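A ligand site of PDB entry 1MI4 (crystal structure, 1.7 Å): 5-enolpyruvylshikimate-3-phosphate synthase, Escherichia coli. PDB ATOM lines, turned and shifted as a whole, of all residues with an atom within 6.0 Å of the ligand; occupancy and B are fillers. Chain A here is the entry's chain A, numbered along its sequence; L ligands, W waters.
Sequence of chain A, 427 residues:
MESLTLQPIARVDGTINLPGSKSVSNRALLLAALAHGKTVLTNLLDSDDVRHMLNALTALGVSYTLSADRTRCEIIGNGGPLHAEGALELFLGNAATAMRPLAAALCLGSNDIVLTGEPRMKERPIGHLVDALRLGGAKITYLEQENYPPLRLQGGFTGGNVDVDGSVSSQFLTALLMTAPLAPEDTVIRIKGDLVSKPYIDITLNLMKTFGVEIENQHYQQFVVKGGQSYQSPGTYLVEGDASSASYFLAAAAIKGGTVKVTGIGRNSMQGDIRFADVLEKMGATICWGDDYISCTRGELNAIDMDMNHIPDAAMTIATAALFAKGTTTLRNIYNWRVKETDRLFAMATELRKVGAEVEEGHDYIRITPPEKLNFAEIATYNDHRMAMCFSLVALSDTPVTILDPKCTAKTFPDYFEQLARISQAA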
ATOM      1  N   LYS A  22     -25.348  12.794  -7.194  1.00  0.00           N
ATOM      2  CA  LYS A  22     -24.323  11.780  -7.417  1.00  0.00           C
ATOM      3  C   LYS A  22     -24.616  10.994  -8.695  1.00  0.00           C
ATOM      4  O   LYS A  22     -23.724  10.755  -9.526  1.00  0.00           O
ATOM      5  CB  LYS A  22     -24.280  10.796  -6.218  1.00  0.00           C
ATOM      6  CG  LYS A  22     -23.290   9.637  -6.480  1.00  0.00           C
ATOM      7  CD  LYS A  22     -24.043   8.258  -6.588  1.00  0.00           C
ATOM      8  CE  LYS A  22     -24.548   7.764  -5.192  1.00  0.00           C
ATOM      9  NZ  LYS A  22     -25.510   6.609  -5.399  1.00  0.00           N
ATOM     10  N   SER A  23     -25.869  10.613  -8.890  1.00  0.00           N
ATOM     11  CA  SER A  23     -26.228   9.843 -10.073  1.00  0.00           C
ATOM     12  C   SER A  23     -25.957  10.590 -11.357  1.00  0.00           C
ATOM     13  O   SER A  23     -25.421  10.032 -12.295  1.00  0.00           O
ATOM     14  CB  SER A  23     -27.707   9.416 -10.029  1.00  0.00           C
ATOM     15  OG  SER A  23     -27.917   8.459  -8.993  1.00  0.00           O
ATOM     16  N   VAL A  24     -26.324  11.879 -11.381  1.00  0.00           N
ATOM     17  CA  VAL A  24     -26.113  12.679 -12.585  1.00  0.00           C
ATOM     18  C   VAL A  24     -24.628  13.012 -12.754  1.00  0.00           C
ATOM     19  O   VAL A  24     -24.067  12.949 -13.865  1.00  0.00           O
ATOM     20  CB  VAL A  24     -26.942  13.973 -12.498  1.00  0.00           C
ATOM     21  CG1 VAL A  24     -26.510  14.952 -13.665  1.00  0.00           C
ATOM     22  CG2 VAL A  24     -28.460  13.607 -12.602  1.00  0.00           C
ATOM     23  N   ARG A  27     -22.545  10.040 -14.185  1.00  0.00           N
ATOM     24  CA  ARG A  27     -22.889   9.772 -15.586  1.00  0.00           C
ATOM     25  C   ARG A  27     -22.312  10.890 -16.464  1.00  0.00           C
ATOM     26  O   ARG A  27     -21.728  10.612 -17.521  1.00  0.00           O
ATOM     27  CB  ARG A  27     -24.420   9.757 -15.791  1.00  0.00           C
ATOM     28  CG  ARG A  27     -25.103   8.460 -15.298  1.00  0.00           C
ATOM     29  CD  ARG A  27     -26.591   8.674 -15.317  1.00  0.00           C
ATOM     30  NE  ARG A  27     -27.397   7.497 -14.987  1.00  0.00           N
ATOM     31  CZ  ARG A  27     -27.509   6.919 -13.790  1.00  0.00           C
ATOM     32  NH1 ARG A  27     -28.312   5.876 -13.658  1.00  0.00           N
ATOM     33  NH2 ARG A  27     -26.848   7.368 -12.730  1.00  0.00           N
ATOM     34  N   THR A  97     -21.744   3.703  -8.994  1.00  0.00           N
ATOM     35  CA  THR A  97     -21.979   4.473 -10.193  1.00  0.00           C
ATOM     36  C   THR A  97     -20.699   4.733 -10.969  1.00  0.00           C
ATOM     37  O   THR A  97     -20.734   5.376 -12.013  1.00  0.00           O
ATOM     38  CB  THR A  97     -22.744   5.783  -9.917  1.00  0.00           C
ATOM     39  OG1 THR A  97     -21.978   6.619  -9.049  1.00  0.00           O
ATOM     40  CG2 THR A  97     -24.104   5.451  -9.309  1.00  0.00           C
ATOM     41  N   ARG A 100     -20.055   0.113 -12.068  1.00  0.00           N
ATOM     42  CA  ARG A 100     -20.822  -0.503 -13.147  1.00  0.00           C
ATOM     43  C   ARG A 100     -20.633   0.187 -14.482  1.00  0.00           C
ATOM     44  O   ARG A 100     -20.388  -0.505 -15.501  1.00  0.00           O
ATOM     45  CB  ARG A 100     -22.318  -0.606 -12.756  1.00  0.00           C
ATOM     46  CG  ARG A 100     -22.676  -1.803 -11.849  1.00  0.00           C
ATOM     47  CD  ARG A 100     -22.095  -1.700 -10.389  1.00  0.00           C
ATOM     48  NE  ARG A 100     -22.557  -2.790  -9.503  1.00  0.00           N
ATOM     49  CZ  ARG A 100     -23.718  -2.756  -8.842  1.00  0.00           C
ATOM     50  NH1 ARG A 100     -24.066  -3.748  -8.044  1.00  0.00           N
ATOM     51  NH2 ARG A 100     -24.575  -1.741  -9.019  1.00  0.00           N
ATOM     52  N   ARG A 124     -20.601  -6.746  -3.743  1.00  0.00           N
ATOM     53  CA  ARG A 124     -21.786  -6.204  -4.428  1.00  0.00           C
ATOM     54  C   ARG A 124     -21.737  -6.811  -5.811  1.00  0.00           C
ATOM     55  O   ARG A 124     -20.743  -6.673  -6.557  1.00  0.00           O
ATOM     56  CB  ARG A 124     -21.726  -4.682  -4.420  1.00  0.00           C
ATOM     57  CG  ARG A 124     -21.810  -4.155  -2.957  1.00  0.00           C
ATOM     58  CD  ARG A 124     -21.806  -2.614  -2.941  1.00  0.00           C
ATOM     59  NE  ARG A 124     -22.996  -2.070  -3.584  1.00  0.00           N
ATOM     60  CZ  ARG A 124     -23.176  -0.786  -3.870  1.00  0.00           C
ATOM     61  NH1 ARG A 124     -24.305  -0.389  -4.464  1.00  0.00           N
ATOM     62  NH2 ARG A 124     -22.253   0.118  -3.556  1.00  0.00           N
ATOM     63  N   VAL A 168     -32.173  -7.289 -10.356  1.00  0.00           N
ATOM     64  CA  VAL A 168     -31.411  -6.963  -9.154  1.00  0.00           C
ATOM     65  C   VAL A 168     -30.936  -5.517  -9.148  1.00  0.00           C
ATOM     66  O   VAL A 168     -30.955  -4.850  -8.111  1.00  0.00           O
ATOM     67  CB  VAL A 168     -30.206  -7.936  -8.984  1.00  0.00           C
ATOM     68  CG1 VAL A 168     -29.288  -7.482  -7.876  1.00  0.00           C
ATOM     69  CG2 VAL A 168     -30.722  -9.336  -8.645  1.00  0.00           C
ATOM     70  N   SER A 169     -30.527  -5.008 -10.302  1.00  0.00           N
ATOM     71  CA  SER A 169     -30.079  -3.610 -10.407  1.00  0.00           C
ATOM     72  C   SER A 169     -30.384  -3.019 -11.772  1.00  0.00           C
ATOM     73  O   SER A 169     -30.309  -3.729 -12.801  1.00  0.00           O
ATOM     74  CB  SER A 169     -28.558  -3.522 -10.181  1.00  0.00           C
ATOM     75  OG  SER A 169     -28.103  -2.162 -10.253  1.00  0.00           O
ATOM     76  N   SER A 170     -30.723  -1.739 -11.792  1.00  0.00           N
ATOM     77  CA  SER A 170     -30.956  -1.044 -13.052  1.00  0.00           C
ATOM     78  C   SER A 170     -29.588  -0.592 -13.587  1.00  0.00           C
ATOM     79  O   SER A 170     -29.474  -0.182 -14.750  1.00  0.00           O
ATOM     80  CB  SER A 170     -31.795   0.230 -12.832  1.00  0.00           C
ATOM     81  OG  SER A 170     -31.118   1.172 -11.986  1.00  0.00           O
ATOM     82  N   GLN A 171     -28.556  -0.639 -12.734  1.00  0.00           N
ATOM     83  CA  GLN A 171     -27.260  -0.135 -13.154  1.00  0.00           C
ATOM     84  C   GLN A 171     -26.583  -0.930 -14.251  1.00  0.00           C
ATOM     85  O   GLN A 171     -25.772  -0.377 -14.986  1.00  0.00           O
ATOM     86  CB  GLN A 171     -26.336  -0.036 -11.950  1.00  0.00           C
ATOM     87  CG  GLN A 171     -26.783   1.008 -10.962  1.00  0.00           C
ATOM     88  CD  GLN A 171     -25.819   1.141  -9.834  1.00  0.00           C
ATOM     89  OE1 GLN A 171     -24.624   0.929 -10.034  1.00  0.00           O
ATOM     90  NE2 GLN A 171     -26.302   1.513  -8.650  1.00  0.00           N
ATOM     91  N   THR A 174     -28.037   0.410 -17.335  1.00  0.00           N
ATOM     92  CA  THR A 174     -27.522   1.767 -17.502  1.00  0.00           C
ATOM     93  C   THR A 174     -26.133   1.722 -18.120  1.00  0.00           C
ATOM     94  O   THR A 174     -25.830   2.436 -19.089  1.00  0.00           O
ATOM     95  CB  THR A 174     -27.477   2.506 -16.152  1.00  0.00           C
ATOM     96  OG1 THR A 174     -28.764   3.084 -15.923  1.00  0.00           O
ATOM     97  CG2 THR A 174     -26.349   3.526 -16.113  1.00  0.00           C
ATOM     98  N   VAL A 196     -35.946  -3.397 -12.049  1.00  0.00           N
ATOM     99  CA  VAL A 196     -36.117  -2.620 -10.846  1.00  0.00           C
ATOM    100  C   VAL A 196     -35.467  -1.256 -11.000  1.00  0.00           C
ATOM    101  O   VAL A 196     -34.719  -1.012 -11.952  1.00  0.00           O
ATOM    102  CB  VAL A 196     -35.489  -3.320  -9.625  1.00  0.00           C
ATOM    103  CG1 VAL A 196     -36.175  -4.654  -9.335  1.00  0.00           C
ATOM    104  CG2 VAL A 196     -34.012  -3.516  -9.870  1.00  0.00           C
ATOM    105  N   SER A 197     -35.794  -0.346 -10.069  1.00  0.00           N
ATOM    106  CA  SER A 197     -35.230   1.003 -10.064  1.00  0.00           C
ATOM    107  C   SER A 197     -35.343   1.650 -11.452  1.00  0.00           C
ATOM    108  O   SER A 197     -34.438   2.357 -11.913  1.00  0.00           O
ATOM    109  CB  SER A 197     -33.756   0.935  -9.640  1.00  0.00           C
ATOM    110  OG  SER A 197     -33.667   0.487  -8.296  1.00  0.00           O
ATOM    111  N   TYR A 200     -34.021   5.210 -12.790  1.00  0.00           N
ATOM    112  CA  TYR A 200     -32.619   5.512 -13.043  1.00  0.00           C
ATOM    113  C   TYR A 200     -32.290   5.298 -14.498  1.00  0.00           C
ATOM    114  O   TYR A 200     -31.293   5.849 -15.014  1.00  0.00           O
ATOM    115  CB  TYR A 200     -31.690   4.685 -12.139  1.00  0.00           C
ATOM    116  CG  TYR A 200     -31.755   5.176 -10.696  1.00  0.00           C
ATOM    117  CD1 TYR A 200     -32.615   4.593  -9.770  1.00  0.00           C
ATOM    118  CD2 TYR A 200     -30.972   6.241 -10.300  1.00  0.00           C
ATOM    119  CE1 TYR A 200     -32.692   5.068  -8.442  1.00  0.00           C
ATOM    120  CE2 TYR A 200     -31.013   6.735  -8.962  1.00  0.00           C
ATOM    121  CZ  TYR A 200     -31.881   6.141  -8.053  1.00  0.00           C
ATOM    122  OH  TYR A 200     -31.925   6.594  -6.739  1.00  0.00           O
ATOM    123  N   ILE A 203     -32.897   8.518 -16.141  1.00  0.00           N
ATOM    124  CA  ILE A 203     -31.806   9.459 -15.895  1.00  0.00           C
ATOM    125  C   ILE A 203     -30.704   9.182 -16.926  1.00  0.00           C
ATOM    126  O   ILE A 203     -30.166  10.104 -17.538  1.00  0.00           O
ATOM    127  CB  ILE A 203     -31.194   9.284 -14.457  1.00  0.00           C
ATOM    128  CG1 ILE A 203     -32.221   9.647 -13.402  1.00  0.00           C
ATOM    129  CG2 ILE A 203     -29.934  10.145 -14.331  1.00  0.00           C
ATOM    130  CD1 ILE A 203     -31.708   9.450 -11.961  1.00  0.00           C
ATOM    131  N   THR A 204     -30.381   7.906 -17.119  1.00  0.00           N
ATOM    132  CA  THR A 204     -29.335   7.555 -18.065  1.00  0.00           C
ATOM    133  C   THR A 204     -29.667   8.038 -19.485  1.00  0.00           C
ATOM    134  O   THR A 204     -28.817   8.641 -20.161  1.00  0.00           O
ATOM    135  CB  THR A 204     -29.153   6.048 -18.064  1.00  0.00           C
ATOM    136  OG1 THR A 204     -28.708   5.678 -16.743  1.00  0.00           O
ATOM    137  CG2 THR A 204     -28.083   5.606 -19.037  1.00  0.00           C
ATOM    138  N   PRO A 312     -35.845   3.436  -4.179  1.00  0.00           N
ATOM    139  CA  PRO A 312     -35.137   2.646  -3.167  1.00  0.00           C
ATOM    140  C   PRO A 312     -34.235   3.396  -2.192  1.00  0.00           C
ATOM    141  O   PRO A 312     -34.199   3.043  -1.033  1.00  0.00           O
ATOM    142  CB  PRO A 312     -34.392   1.623  -3.992  1.00  0.00           C
ATOM    143  CG  PRO A 312     -34.102   2.350  -5.307  1.00  0.00           C
ATOM    144  CD  PRO A 312     -35.448   3.029  -5.546  1.00  0.00           C
ATOM    145  N   ASP A 313     -33.518   4.405  -2.669  1.00  0.00           N
ATOM    146  CA  ASP A 313     -32.613   5.155  -1.787  1.00  0.00           C
ATOM    147  C   ASP A 313     -33.385   6.077  -0.843  1.00  0.00           C
ATOM    148  O   ASP A 313     -33.245   6.016   0.381  1.00  0.00           O
ATOM    149  CB  ASP A 313     -31.606   5.969  -2.612  1.00  0.00           C
ATOM    150  CG  ASP A 313     -30.584   5.105  -3.356  1.00  0.00           C
ATOM    151  OD1 ASP A 313     -29.841   5.676  -4.191  1.00  0.00           O
ATOM    152  OD2 ASP A 313     -30.533   3.869  -3.143  1.00  0.00           O
ATOM    153  N   ASN A 336     -33.456  -5.221  -3.191  1.00  0.00           N
ATOM    154  CA  ASN A 336     -32.073  -4.840  -3.469  1.00  0.00           C
ATOM    155  C   ASN A 336     -31.399  -3.931  -2.473  1.00  0.00           C
ATOM    156  O   ASN A 336     -30.218  -3.609  -2.624  1.00  0.00           O
ATOM    157  CB  ASN A 336     -31.858  -4.407  -4.959  1.00  0.00           C
ATOM    158  CG  ASN A 336     -32.325  -3.026  -5.265  1.00  0.00           C
ATOM    159  OD1 ASN A 336     -32.658  -2.228  -4.378  1.00  0.00           O
ATOM    160  ND2 ASN A 336     -32.304  -2.689  -6.577  1.00  0.00           N
ATOM    161  N   LYS A 340     -26.608  -3.313  -1.526  1.00  0.00           N
ATOM    162  CA  LYS A 340     -26.067  -1.980  -1.729  1.00  0.00           C
ATOM    163  C   LYS A 340     -24.932  -1.634  -0.767  1.00  0.00           C
ATOM    164  O   LYS A 340     -24.136  -2.504  -0.461  1.00  0.00           O
ATOM    165  CB  LYS A 340     -27.221  -0.975  -1.704  1.00  0.00           C
ATOM    166  CG  LYS A 340     -27.925  -1.068  -3.061  1.00  0.00           C
ATOM    167  CD  LYS A 340     -29.282  -0.436  -3.024  1.00  0.00           C
ATOM    168  CE  LYS A 340     -29.782  -0.465  -4.462  1.00  0.00           C
ATOM    169  NZ  LYS A 340     -31.066   0.258  -4.632  1.00  0.00           N
ATOM    170  N   GLU A 341     -24.828  -0.387  -0.320  1.00  0.00           N
ATOM    171  CA  GLU A 341     -23.683  -0.046   0.543  1.00  0.00           C
ATOM    172  C   GLU A 341     -23.492  -1.014   1.696  1.00  0.00           C
ATOM    173  O   GLU A 341     -22.372  -1.270   2.122  1.00  0.00           O
ATOM    174  CB  GLU A 341     -23.790   1.408   1.012  1.00  0.00           C
ATOM    175  CG  GLU A 341     -23.335   2.388  -0.098  1.00  0.00           C
ATOM    176  CD  GLU A 341     -24.390   2.777  -1.105  1.00  0.00           C
ATOM    177  OE1 GLU A 341     -25.289   1.959  -1.452  1.00  0.00           O
ATOM    178  OE2 GLU A 341     -24.292   3.915  -1.593  1.00  0.00           O
ATOM    179  N   ARG A 344     -29.134  -3.204   3.598  1.00  0.00           N
ATOM    180  CA  ARG A 344     -29.907  -2.169   4.240  1.00  0.00           C
ATOM    181  C   ARG A 344     -31.162  -2.643   4.943  1.00  0.00           C
ATOM    182  O   ARG A 344     -31.655  -1.961   5.815  1.00  0.00           O
ATOM    183  CB  ARG A 344     -30.207  -1.051   3.224  1.00  0.00           C
ATOM    184  CG  ARG A 344     -28.933  -0.234   2.862  1.00  0.00           C
ATOM    185  CD  ARG A 344     -29.105   0.606   1.605  1.00  0.00           C
ATOM    186  NE  ARG A 344     -28.105   1.691   1.593  1.00  0.00           N
ATOM    187  CZ  ARG A 344     -27.979   2.583   0.621  1.00  0.00           C
ATOM    188  NH1 ARG A 344     -27.063   3.561   0.719  1.00  0.00           N
ATOM    189  NH2 ARG A 344     -28.750   2.495  -0.473  1.00  0.00           N
ATOM    190  N   ARG A 386     -26.205   6.638   3.991  1.00  0.00           N
ATOM    191  CA  ARG A 386     -27.640   6.807   4.268  1.00  0.00           C
ATOM    192  C   ARG A 386     -28.076   6.295   5.637  1.00  0.00           C
ATOM    193  O   ARG A 386     -29.064   6.749   6.174  1.00  0.00           O
ATOM    194  CB  ARG A 386     -28.459   6.140   3.166  1.00  0.00           C
ATOM    195  CG  ARG A 386     -28.134   6.721   1.793  1.00  0.00           C
ATOM    196  CD  ARG A 386     -29.341   6.570   0.818  1.00  0.00           C
ATOM    197  NE  ARG A 386     -28.854   7.057  -0.479  1.00  0.00           N
ATOM    198  CZ  ARG A 386     -28.645   8.332  -0.792  1.00  0.00           C
ATOM    199  NH1 ARG A 386     -28.140   8.606  -1.993  1.00  0.00           N
ATOM    200  NH2 ARG A 386     -29.045   9.331   0.018  1.00  0.00           N
HETATM  201  C1  LIG L   1     -28.356   4.405  -9.022  1.00  0.00           C
HETATM  202  C2  LIG L   1     -29.338   3.377  -9.142  1.00  0.00           C
HETATM  203  C3  LIG L   1     -29.837   2.641  -7.918  1.00  0.00           C
HETATM  204  C4  LIG L   1     -29.545   3.409  -6.611  1.00  0.00           C
HETATM  205  C5  LIG L   1     -28.049   3.799  -6.564  1.00  0.00           C
HETATM  206  C6  LIG L   1     -27.814   4.800  -7.716  1.00  0.00           C
HETATM  207  C7  LIG L   1     -27.881   5.090 -10.270  1.00  0.00           C
HETATM  208  O1  LIG L   1     -29.307   1.315  -7.855  1.00  0.00           O
HETATM  209  O2  LIG L   1     -29.898   2.557  -5.525  1.00  0.00           O
HETATM  210  O3  LIG L   1     -27.735   4.430  -5.322  1.00  0.00           O
HETATM  211  O4  LIG L   1     -27.948   4.453 -11.355  1.00  0.00           O
HETATM  212  O5  LIG L   1     -27.448   6.219 -10.164  1.00  0.00           O
HETATM  213  P1  LIG L   1     -30.071  -0.004  -8.255  1.00  0.00           P
HETATM  214  O6  LIG L   1     -30.389   0.096  -9.696  1.00  0.00           O
HETATM  215  O7  LIG L   1     -31.356  -0.094  -7.421  1.00  0.00           O
HETATM  216  O8  LIG L   1     -29.146  -1.170  -8.035  1.00  0.00           O
HETATM  217  O   HOH W   1     -29.070   2.784 -13.297  1.00  0.00           O
HETATM  218  O   HOH W   2     -26.627  -1.207  -7.021  1.00  0.00           O
HETATM  219  O   HOH W   3     -26.993   2.010  -3.660  1.00  0.00           O
HETATM  220  O   HOH W   4     -28.983  -3.557  -6.713  1.00  0.00           O
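Water W2 lies within hydrogen-bond range of an oxygen (O8) of the ligand (2.7 Å), the guanidinium group of Arg 100 (2.9 Å) and the side-chain amide nitrogen of Gln 171 (3.2 Å). Water W4 lies within hydrogen-bond range of an oxygen (O8) of the ligand (2.7 Å), the backbone carbonyl oxygen of Val 168 (2.7 Å) and the side-chain amide nitrogen of Asn 336 (3.4 Å). Water W1 lies within hydrogen-bond range of the side-chain hydroxyl of Thr 174 (2.7 Å), an oxygen (O4) of the ligand (2.8 Å), the side-chain hydroxyl of Ser 170 (2.9 Å) and the guanidinium group of Arg 27 (3.2 Å). Water W3 bridges OE1 of Glu 341 (2.8 Å) and O3 of the ligand (3.0 Å).
The side-chain carboxylate of Asp 313 sits at hydrogen-bond distance from the side-chain hydroxyl of Tyr 200 (3.4 Å). OD1 of Asn 336 is in hydrogen-bond range of NZ of Lys 340 (3.0 Å). The side-chain amide oxygen (OE1) of Gln 171 is in hydrogen-bond range of the guanidinium group (NH2) of Arg 100 (2.9 Å). OD2 of Asp 313 is in salt-bridge range of NH2 of Arg 344. NZ of Lys 340 is in salt-bridge range of OD2 of Asp 313. NH1 of Arg 27 sits at hydrogen-bond distance from O of Tyr 200. The backbone NH (N) of Gln 171 is in hydrogen-bond range of the side-chain hydroxyl (OG) of Ser 169. O of Ser 23 is in hydrogen-bond range of NH2 of Arg 27, at 3.1 Å.
Residues that only touch the ligand: Thr 97 and Tyr 200. Within 4 Å of the ligand: Lys 22, Ser 23, Arg 27, Thr 97, Ser 169, Ser 170, Gln 171, Ser 197, Tyr 200, Asp 313, Asn 336 and Lys 340. Along chain A the residues within 4 Å of the ligand span positions 22 to 340.
An oxygen (O6) of the ligand lies within hydrogen-bond range of the backbone NH (N) of Ser 170 (2.8 Å). An oxygen (O3) of the ligand lies within hydrogen-bond range of the side-chain amino group of Lys 22, 3.1 Å away. An oxygen (O4) of the ligand lies within salt-bridge range of the guanidinium group (NH1) of Arg 27, 2.7 Å away. NE2 of Gln 171 lies within hydrogen-bond range of O1 of the ligand, at 3.1 Å. The side-chain carboxylate (OD1) of Asp 313 lies within hydrogen-bond range of an oxygen (O3) of the ligand (2.7 Å). OG of Ser 23 is in hydrogen-bond range of O5 of the ligand (2.6 Å). OG of Ser 197 sits at hydrogen-bond distance from O7 of the ligand, at 2.5 Å. The side-chain hydroxyl of Ser 169 lies within hydrogen-bond range of an oxygen (O8) of the ligand, at 2.6 Å. ND2 of Asn 336 lies within hydrogen-bond range of O7 of the ligand. The side-chain hydroxyl (OG) of Ser 170 lies within hydrogen-bond range of an oxygen (O6) of the ligand (2.6 Å). NZ of Lys 340 lies within salt-bridge range of O7 of the ligand (2.8 Å).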
